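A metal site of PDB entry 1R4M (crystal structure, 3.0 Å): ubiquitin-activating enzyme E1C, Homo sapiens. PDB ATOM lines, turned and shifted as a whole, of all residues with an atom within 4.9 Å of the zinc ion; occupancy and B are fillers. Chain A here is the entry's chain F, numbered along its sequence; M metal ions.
The backbone NH of Glu 190 lies close to the side-chain sulfur of Cys 188.
Of the 7 residues printed, 4 come within 4 Å of the zinc ion.
The zinc ion is bound by the side-chain sulfur of Cys 335 (2.1 Å), the side-chain sulfur of Cys 332 (2.1 Å), the side-chain sulfur of Cys 191 (2.2 Å) and the side-chain sulfur of Cys 188 (2.2 Å).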
ATOM      1  N   CYS A 188      27.963 -22.990   3.568  1.00  0.00           N
ATOM      2  CA  CYS A 188      28.002 -23.857   2.403  1.00  0.00           C
ATOM      3  C   CYS A 188      26.617 -24.037   1.775  1.00  0.00           C
ATOM      4  O   CYS A 188      25.627 -23.491   2.256  1.00  0.00           O
ATOM      5  CB  CYS A 188      28.574 -25.236   2.773  1.00  0.00           C
ATOM      6  SG  CYS A 188      27.446 -26.293   3.704  1.00  0.00           S
ATOM      7  N   GLU A 190      24.918 -26.653   1.782  1.00  0.00           N
ATOM      8  CA  GLU A 190      24.167 -27.427   2.760  1.00  0.00           C
ATOM      9  C   GLU A 190      23.619 -26.470   3.828  1.00  0.00           C
ATOM     10  O   GLU A 190      22.435 -26.509   4.155  1.00  0.00           O
ATOM     11  CB  GLU A 190      25.099 -28.478   3.380  1.00  0.00           C
ATOM     12  CG  GLU A 190      24.532 -29.900   3.511  1.00  0.00           C
ATOM     13  CD  GLU A 190      24.024 -30.473   2.195  1.00  0.00           C
ATOM     14  OE1 GLU A 190      22.832 -30.288   1.901  1.00  0.00           O
ATOM     15  OE2 GLU A 190      24.817 -31.097   1.446  1.00  0.00           O
ATOM     16  N   CYS A 191      24.500 -25.602   4.351  1.00  0.00           N
ATOM     17  CA  CYS A 191      24.114 -24.638   5.366  1.00  0.00           C
ATOM     18  C   CYS A 191      22.811 -23.917   5.025  1.00  0.00           C
ATOM     19  O   CYS A 191      21.968 -23.673   5.887  1.00  0.00           O
ATOM     20  CB  CYS A 191      25.206 -23.595   5.557  1.00  0.00           C
ATOM     21  SG  CYS A 191      26.742 -24.208   6.231  1.00  0.00           S
ATOM     22  N   LYS A 329      25.598 -22.407   9.493  1.00  0.00           N
ATOM     23  CA  LYS A 329      25.160 -23.303  10.567  1.00  0.00           C
ATOM     24  C   LYS A 329      26.374 -23.999  11.157  1.00  0.00           C
ATOM     25  O   LYS A 329      27.151 -24.616  10.433  1.00  0.00           O
ATOM     26  CB  LYS A 329      24.172 -24.349  10.036  1.00  0.00           C
ATOM     27  CG  LYS A 329      22.842 -23.777   9.612  1.00  0.00           C
ATOM     28  CD  LYS A 329      21.800 -24.871   9.508  1.00  0.00           C
ATOM     29  CE  LYS A 329      20.430 -24.270   9.205  1.00  0.00           C
ATOM     30  NZ  LYS A 329      19.320 -25.283   9.146  1.00  0.00           N
ATOM     31  N   CYS A 332      26.368 -27.808  10.630  1.00  0.00           N
ATOM     32  CA  CYS A 332      26.170 -28.235   9.252  1.00  0.00           C
ATOM     33  C   CYS A 332      26.737 -29.634   9.104  1.00  0.00           C
ATOM     34  O   CYS A 332      27.929 -29.856   9.297  1.00  0.00           O
ATOM     35  CB  CYS A 332      26.873 -27.283   8.284  1.00  0.00           C
ATOM     36  SG  CYS A 332      26.253 -27.420   6.589  1.00  0.00           S
ATOM     37  N   ALA A 334      27.505 -31.105   6.701  1.00  0.00           N
ATOM     38  CA  ALA A 334      28.525 -31.018   5.671  1.00  0.00           C
ATOM     39  C   ALA A 334      29.788 -30.230   6.003  1.00  0.00           C
ATOM     40  O   ALA A 334      30.861 -30.819   6.055  1.00  0.00           O
ATOM     41  CB  ALA A 334      27.903 -30.461   4.418  1.00  0.00           C
ATOM     42  N   CYS A 335      29.694 -28.917   6.206  1.00  0.00           N
ATOM     43  CA  CYS A 335      30.891 -28.129   6.505  1.00  0.00           C
ATOM     44  C   CYS A 335      31.313 -28.057   7.981  1.00  0.00           C
ATOM     45  O   CYS A 335      32.207 -27.295   8.318  1.00  0.00           O
ATOM     46  CB  CYS A 335      30.757 -26.696   5.957  1.00  0.00           C
ATOM     47  SG  CYS A 335      29.536 -25.648   6.748  1.00  0.00           S
HETATM   48 ZN    ZN M   1      27.744 -26.135   5.878  1.00  0.00          ZN
